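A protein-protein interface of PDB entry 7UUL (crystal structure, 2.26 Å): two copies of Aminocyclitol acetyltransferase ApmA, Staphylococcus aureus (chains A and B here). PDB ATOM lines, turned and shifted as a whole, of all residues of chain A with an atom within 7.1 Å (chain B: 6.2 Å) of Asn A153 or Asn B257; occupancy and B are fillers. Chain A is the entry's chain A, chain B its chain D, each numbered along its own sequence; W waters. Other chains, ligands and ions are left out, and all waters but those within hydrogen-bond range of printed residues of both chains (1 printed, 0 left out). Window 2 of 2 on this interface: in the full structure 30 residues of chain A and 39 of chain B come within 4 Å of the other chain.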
ATOM      1  N   GLN A 149     -18.308  14.746   1.184  1.00  0.00           N
ATOM      2  CA  GLN A 149     -17.441  15.893   1.421  1.00  0.00           C
ATOM      3  C   GLN A 149     -17.431  16.330   2.878  1.00  0.00           C
ATOM      4  O   GLN A 149     -16.490  17.011   3.299  1.00  0.00           O
ATOM      5  CB  GLN A 149     -17.847  17.071   0.533  1.00  0.00           C
ATOM      6  CG  GLN A 149     -19.048  17.858   1.008  1.00  0.00           C
ATOM      7  CD  GLN A 149     -19.564  18.794  -0.065  1.00  0.00           C
ATOM      8  OE1 GLN A 149     -20.761  18.837  -0.336  1.00  0.00           O
ATOM      9  NE2 GLN A 149     -18.666  19.532  -0.697  1.00  0.00           N
ATOM     10  N   ASN A 150     -18.433  15.947   3.663  1.00  0.00           N
ATOM     11  CA  ASN A 150     -18.359  16.222   5.089  1.00  0.00           C
ATOM     12  C   ASN A 150     -17.157  15.543   5.721  1.00  0.00           C
ATOM     13  O   ASN A 150     -16.728  15.945   6.806  1.00  0.00           O
ATOM     14  CB  ASN A 150     -19.654  15.782   5.786  1.00  0.00           C
ATOM     15  CG  ASN A 150     -20.856  16.605   5.349  1.00  0.00           C
ATOM     16  OD1 ASN A 150     -20.714  17.725   4.842  1.00  0.00           O
ATOM     17  ND2 ASN A 150     -22.051  16.050   5.532  1.00  0.00           N
ATOM     18  N   PHE A 151     -16.597  14.529   5.064  1.00  0.00           N
ATOM     19  CA  PHE A 151     -15.417  13.841   5.564  1.00  0.00           C
ATOM     20  C   PHE A 151     -14.123  14.379   4.969  1.00  0.00           C
ATOM     21  O   PHE A 151     -13.044  13.962   5.394  1.00  0.00           O
ATOM     22  CB  PHE A 151     -15.539  12.336   5.295  1.00  0.00           C
ATOM     23  CG  PHE A 151     -16.460  11.608   6.252  1.00  0.00           C
ATOM     24  CD1 PHE A 151     -16.845  12.188   7.449  1.00  0.00           C
ATOM     25  CD2 PHE A 151     -16.930  10.342   5.952  1.00  0.00           C
ATOM     26  CE1 PHE A 151     -17.673  11.522   8.326  1.00  0.00           C
ATOM     27  CE2 PHE A 151     -17.763   9.666   6.831  1.00  0.00           C
ATOM     28  CZ  PHE A 151     -18.137  10.266   8.018  1.00  0.00           C
ATOM     29  N   PHE A 152     -14.199  15.313   4.023  1.00  0.00           N
ATOM     30  CA  PHE A 152     -13.019  15.813   3.325  1.00  0.00           C
ATOM     31  C   PHE A 152     -12.260  16.835   4.175  1.00  0.00           C
ATOM     32  O   PHE A 152     -12.863  17.779   4.700  1.00  0.00           O
ATOM     33  CB  PHE A 152     -13.435  16.455   1.995  1.00  0.00           C
ATOM     34  CG  PHE A 152     -13.817  15.468   0.919  1.00  0.00           C
ATOM     35  CD1 PHE A 152     -13.491  14.121   1.034  1.00  0.00           C
ATOM     36  CD2 PHE A 152     -14.469  15.898  -0.223  1.00  0.00           C
ATOM     37  CE1 PHE A 152     -13.840  13.209   0.033  1.00  0.00           C
ATOM     38  CE2 PHE A 152     -14.831  15.008  -1.219  1.00  0.00           C
ATOM     39  CZ  PHE A 152     -14.519  13.649  -1.099  1.00  0.00           C
ATOM     40  N   ASN A 153     -10.936  16.664   4.298  1.00  0.00           N
ATOM     41  CA  ASN A 153     -10.126  17.705   4.920  1.00  0.00           C
ATOM     42  C   ASN A 153      -9.924  18.865   3.944  1.00  0.00           C
ATOM     43  O   ASN A 153     -10.395  18.849   2.802  1.00  0.00           O
ATOM     44  CB  ASN A 153      -8.787  17.154   5.420  1.00  0.00           C
ATOM     45  CG  ASN A 153      -7.895  16.586   4.299  1.00  0.00           C
ATOM     46  OD1 ASN A 153      -8.058  16.900   3.116  1.00  0.00           O
ATOM     47  ND2 ASN A 153      -6.937  15.744   4.689  1.00  0.00           N
ATOM     48  N   GLU A 154      -9.211  19.891   4.400  1.00  0.00           N
ATOM     49  CA  GLU A 154      -9.022  21.081   3.574  1.00  0.00           C
ATOM     50  C   GLU A 154      -8.474  20.716   2.200  1.00  0.00           C
ATOM     51  O   GLU A 154      -8.949  21.223   1.174  1.00  0.00           O
ATOM     52  CB  GLU A 154      -8.083  22.060   4.284  1.00  0.00           C
ATOM     53  CG  GLU A 154      -8.781  22.997   5.238  1.00  0.00           C
ATOM     54  CD  GLU A 154      -8.116  24.364   5.298  1.00  0.00           C
ATOM     55  OE1 GLU A 154      -6.910  24.424   5.618  1.00  0.00           O
ATOM     56  OE2 GLU A 154      -8.798  25.375   5.015  1.00  0.00           O
ATOM     57  N   GLU A 155      -7.506  19.805   2.157  1.00  0.00           N
ATOM     58  CA  GLU A 155      -6.858  19.479   0.893  1.00  0.00           C
ATOM     59  C   GLU A 155      -7.761  18.631   0.010  1.00  0.00           C
ATOM     60  O   GLU A 155      -7.925  18.929  -1.180  1.00  0.00           O
ATOM     61  CB  GLU A 155      -5.528  18.790   1.163  1.00  0.00           C
ATOM     62  CG  GLU A 155      -4.671  19.615   2.121  1.00  0.00           C
ATOM     63  CD  GLU A 155      -4.680  19.047   3.534  1.00  0.00           C
ATOM     64  OE1 GLU A 155      -3.895  18.084   3.808  1.00  0.00           O
ATOM     65  OE2 GLU A 155      -5.461  19.593   4.364  1.00  0.00           O
ATOM     66  N   SER A 156      -8.382  17.585   0.573  1.00  0.00           N
ATOM     67  CA  SER A 156      -9.331  16.811  -0.224  1.00  0.00           C
ATOM     68  C   SER A 156     -10.430  17.710  -0.765  1.00  0.00           C
ATOM     69  O   SER A 156     -10.827  17.593  -1.930  1.00  0.00           O
ATOM     70  CB  SER A 156      -9.947  15.662   0.584  1.00  0.00           C
ATOM     71  OG  SER A 156      -8.970  14.912   1.280  1.00  0.00           O
ATOM     72  N   MET A 157     -10.915  18.643   0.051  1.00  0.00           N
ATOM     73  CA  MET A 157     -12.041  19.413  -0.439  1.00  0.00           C
ATOM     74  C   MET A 157     -11.603  20.366  -1.549  1.00  0.00           C
ATOM     75  O   MET A 157     -12.354  20.582  -2.509  1.00  0.00           O
ATOM     76  CB  MET A 157     -12.734  20.177   0.691  1.00  0.00           C
ATOM     77  CG  MET A 157     -13.559  21.280   0.111  1.00  0.00           C
ATOM     78  SD  MET A 157     -15.180  20.505  -0.102  1.00  0.00           S
ATOM     79  CE  MET A 157     -15.682  20.186   1.600  1.00  0.00           C
ATOM     80  N   ALA A 158     -10.366  20.864  -1.482  1.00  0.00           N
ATOM     81  CA  ALA A 158      -9.873  21.775  -2.510  1.00  0.00           C
ATOM     82  C   ALA A 158      -9.818  21.102  -3.880  1.00  0.00           C
ATOM     83  O   ALA A 158     -10.277  21.675  -4.878  1.00  0.00           O
ATOM     84  CB  ALA A 158      -8.498  22.316  -2.119  1.00  0.00           C
ATOM     85  N   VAL A 159      -9.248  19.893  -3.957  1.00  0.00           N
ATOM     86  CA  VAL A 159      -9.216  19.199  -5.245  1.00  0.00           C
ATOM     87  C   VAL A 159     -10.632  18.869  -5.701  1.00  0.00           C
ATOM     88  O   VAL A 159     -10.959  19.003  -6.884  1.00  0.00           O
ATOM     89  CB  VAL A 159      -8.319  17.942  -5.191  1.00  0.00           C
ATOM     90  CG1 VAL A 159      -6.849  18.327  -5.085  1.00  0.00           C
ATOM     91  CG2 VAL A 159      -8.681  17.058  -4.042  1.00  0.00           C
ATOM     92  N   SER B 252     -12.213   4.210   6.110  1.00  0.00           N
ATOM     93  CA  SER B 252     -12.146   5.151   7.211  1.00  0.00           C
ATOM     94  C   SER B 252     -12.061   6.576   6.669  1.00  0.00           C
ATOM     95  O   SER B 252     -11.700   6.804   5.515  1.00  0.00           O
ATOM     96  CB  SER B 252     -10.943   4.839   8.103  1.00  0.00           C
ATOM     97  OG  SER B 252      -9.726   5.205   7.477  1.00  0.00           O
ATOM     98  N   ILE B 253     -12.425   7.545   7.513  1.00  0.00           N
ATOM     99  CA  ILE B 253     -12.249   8.942   7.129  1.00  0.00           C
ATOM    100  C   ILE B 253     -10.814   9.182   6.693  1.00  0.00           C
ATOM    101  O   ILE B 253     -10.554   9.845   5.684  1.00  0.00           O
ATOM    102  CB  ILE B 253     -12.641   9.876   8.286  1.00  0.00           C
ATOM    103  CG1 ILE B 253     -14.158   9.896   8.469  1.00  0.00           C
ATOM    104  CG2 ILE B 253     -12.091  11.282   8.042  1.00  0.00           C
ATOM    105  CD1 ILE B 253     -14.555  10.138   9.904  1.00  0.00           C
ATOM    106  N   GLU B 254      -9.861   8.618   7.434  1.00  0.00           N
ATOM    107  CA  GLU B 254      -8.455   8.793   7.090  1.00  0.00           C
ATOM    108  C   GLU B 254      -8.169   8.231   5.705  1.00  0.00           C
ATOM    109  O   GLU B 254      -7.490   8.870   4.894  1.00  0.00           O
ATOM    110  CB  GLU B 254      -7.576   8.118   8.151  1.00  0.00           C
ATOM    111  CG  GLU B 254      -7.599   8.800   9.536  1.00  0.00           C
ATOM    112  CD  GLU B 254      -9.024   8.976  10.125  1.00  0.00           C
ATOM    113  OE1 GLU B 254      -9.735   7.958  10.350  1.00  0.00           O
ATOM    114  OE2 GLU B 254      -9.433  10.146  10.342  1.00  0.00           O
ATOM    115  N   GLU B 255      -8.716   7.049   5.405  1.00  0.00           N
ATOM    116  CA  GLU B 255      -8.502   6.438   4.099  1.00  0.00           C
ATOM    117  C   GLU B 255      -9.150   7.254   2.982  1.00  0.00           C
ATOM    118  O   GLU B 255      -8.593   7.367   1.882  1.00  0.00           O
ATOM    119  CB  GLU B 255      -9.034   5.010   4.104  1.00  0.00           C
ATOM    120  CG  GLU B 255      -8.155   4.059   4.875  1.00  0.00           C
ATOM    121  CD  GLU B 255      -8.800   2.718   5.079  1.00  0.00           C
ATOM    122  OE1 GLU B 255      -9.940   2.682   5.587  1.00  0.00           O
ATOM    123  OE2 GLU B 255      -8.177   1.699   4.709  1.00  0.00           O
ATOM    124  N   ILE B 256     -10.322   7.836   3.239  1.00  0.00           N
ATOM    125  CA  ILE B 256     -10.957   8.653   2.210  1.00  0.00           C
ATOM    126  C   ILE B 256     -10.070   9.837   1.855  1.00  0.00           C
ATOM    127  O   ILE B 256      -9.947  10.220   0.684  1.00  0.00           O
ATOM    128  CB  ILE B 256     -12.353   9.096   2.670  1.00  0.00           C
ATOM    129  CG1 ILE B 256     -13.309   7.907   2.584  1.00  0.00           C
ATOM    130  CG2 ILE B 256     -12.853  10.297   1.856  1.00  0.00           C
ATOM    131  CD1 ILE B 256     -14.519   8.029   3.487  1.00  0.00           C
ATOM    132  N   ASN B 257      -9.404  10.410   2.849  1.00  0.00           N
ATOM    133  CA  ASN B 257      -8.520  11.522   2.536  1.00  0.00           C
ATOM    134  C   ASN B 257      -7.202  11.044   1.948  1.00  0.00           C
ATOM    135  O   ASN B 257      -6.670  11.684   1.039  1.00  0.00           O
ATOM    136  CB  ASN B 257      -8.307  12.383   3.777  1.00  0.00           C
ATOM    137  CG  ASN B 257      -9.576  13.135   4.171  1.00  0.00           C
ATOM    138  OD1 ASN B 257      -9.968  14.104   3.504  1.00  0.00           O
ATOM    139  ND2 ASN B 257     -10.239  12.676   5.239  1.00  0.00           N
ATOM    140  N   GLU B 258      -6.677   9.912   2.426  1.00  0.00           N
ATOM    141  CA  GLU B 258      -5.421   9.398   1.886  1.00  0.00           C
ATOM    142  C   GLU B 258      -5.560   9.066   0.406  1.00  0.00           C
ATOM    143  O   GLU B 258      -4.636   9.290  -0.385  1.00  0.00           O
ATOM    144  CB  GLU B 258      -4.973   8.167   2.678  1.00  0.00           C
ATOM    145  CG  GLU B 258      -4.105   8.481   3.893  1.00  0.00           C
ATOM    146  CD  GLU B 258      -3.949   7.295   4.881  1.00  0.00           C
ATOM    147  OE1 GLU B 258      -4.741   6.310   4.822  1.00  0.00           O
ATOM    148  OE2 GLU B 258      -3.025   7.363   5.734  1.00  0.00           O
ATOM    149  N   ASN B 259      -6.716   8.555   0.002  1.00  0.00           N
ATOM    150  CA  ASN B 259      -6.898   8.083  -1.361  1.00  0.00           C
ATOM    151  C   ASN B 259      -7.884   8.940  -2.148  1.00  0.00           C
ATOM    152  O   ASN B 259      -8.479   8.456  -3.114  1.00  0.00           O
ATOM    153  CB  ASN B 259      -7.350   6.621  -1.348  1.00  0.00           C
ATOM    154  CG  ASN B 259      -6.363   5.709  -0.640  1.00  0.00           C
ATOM    155  OD1 ASN B 259      -5.286   5.421  -1.155  1.00  0.00           O
ATOM    156  ND2 ASN B 259      -6.733   5.244   0.535  1.00  0.00           N
ATOM    157  N   VAL B 260      -8.058  10.210  -1.763  1.00  0.00           N
ATOM    158  CA  VAL B 260      -9.054  11.057  -2.421  1.00  0.00           C
ATOM    159  C   VAL B 260      -8.752  11.202  -3.906  1.00  0.00           C
ATOM    160  O   VAL B 260      -9.674  11.348  -4.725  1.00  0.00           O
ATOM    161  CB  VAL B 260      -9.134  12.430  -1.727  1.00  0.00           C
ATOM    162  CG1 VAL B 260      -7.798  13.192  -1.852  1.00  0.00           C
ATOM    163  CG2 VAL B 260     -10.281  13.238  -2.305  1.00  0.00           C
ATOM    164  N   ASP B 261      -7.466  11.142  -4.280  1.00  0.00           N
ATOM    165  CA  ASP B 261      -7.107  11.221  -5.692  1.00  0.00           C
ATOM    166  C   ASP B 261      -7.813  10.136  -6.491  1.00  0.00           C
ATOM    167  O   ASP B 261      -8.306  10.388  -7.596  1.00  0.00           O
ATOM    168  CB  ASP B 261      -5.583  11.133  -5.873  1.00  0.00           C
ATOM    169  CG  ASP B 261      -4.946   9.899  -5.190  1.00  0.00           C
ATOM    170  OD1 ASP B 261      -5.665   9.021  -4.651  1.00  0.00           O
ATOM    171  OD2 ASP B 261      -3.694   9.801  -5.205  1.00  0.00           O
ATOM    172  N   LEU B 263     -10.630   8.656  -5.469  1.00  0.00           N
ATOM    173  CA  LEU B 263     -12.063   8.917  -5.424  1.00  0.00           C
ATOM    174  C   LEU B 263     -12.453   9.962  -6.460  1.00  0.00           C
ATOM    175  O   LEU B 263     -13.539   9.890  -7.052  1.00  0.00           O
ATOM    176  CB  LEU B 263     -12.485   9.366  -4.021  1.00  0.00           C
ATOM    177  CG  LEU B 263     -12.305   8.320  -2.922  1.00  0.00           C
ATOM    178  CD1 LEU B 263     -12.711   8.851  -1.563  1.00  0.00           C
ATOM    179  CD2 LEU B 263     -13.111   7.089  -3.276  1.00  0.00           C
HETATM  180  O   HOH W   1      -6.266  14.740   0.508  1.00  0.00           O
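Water W1 bridges OG of Ser A156 and O of Asn B257.
CG of Phe A151 touches CG1 of Ile B253 (3.6 Å).
CG2 of Ile B256 touches CE1 of Phe A152, at 3.6 Å.
CA of Phe A152 touches OD1 of Asn B257 (3.5 Å).
CG1 of Val B260 touches OG of Ser A156 (3.8 Å).
Of the printed residues of chain B, Phe A151 touches Ile B253 and Asn B257.
Of chain B, only Asn B257 (2.8 Å) comes within 4 Å of Asn A153.
Glu A154 touches none of the printed residues of chain B.
Ala A158 touches none of the printed residues of chain B.
Of the printed residues of chain A, Ile B256 touches Phe A152.
Of chain A, only Phe A151, Phe A152, Asn A153 and Ser A156 come within 4 Å of Asn B257.
The nearest printed residue of chain B that does not touch Ser A156 is Ile B256 (4.8 Å).
Of the 11 printed residues of chain A, 4 touch a printed residue of chain B.
Hydrophobic or aromatic side chains of chain A within 4 Å of the printed part of chain B: Phe A151 and Phe A152.
Among the printed residues, 7 pairs touch across the chains.
Among the printed residues, no Asp or Glu carboxylate lies within 4 Å of a Lys or Arg side-chain nitrogen of the other chain.
No position is printed for both chains.
Of the 7 pairs that touch across the chains among the printed residues, none has its exchanged pair printed and touching as well.
ND2 of Asn B257 sits at hydrogen-bond distance from O of Phe A151 (3.1 Å).
The side-chain amide oxygen of Asn B257 is in hydrogen-bond range of the backbone NH of Asn A153 (2.8 Å).
The side-chain amide oxygen (OD1) of Asn B257 is in hydrogen-bond range of the side-chain hydroxyl (OG) of Ser A156 (2.6 Å).
The side-chain amide oxygen (OD1) of Asn A153 sits at hydrogen-bond distance from the backbone NH (N) of Ser A156 (2.7 Å).
O of Ile B253 lies within hydrogen-bond range of ND2 of Asn B257 (2.9 Å).
The side-chain amide oxygen (OD1) of Asn A153 sits at hydrogen-bond distance from the backbone NH (N) of Glu A155, at 3.1 Å.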
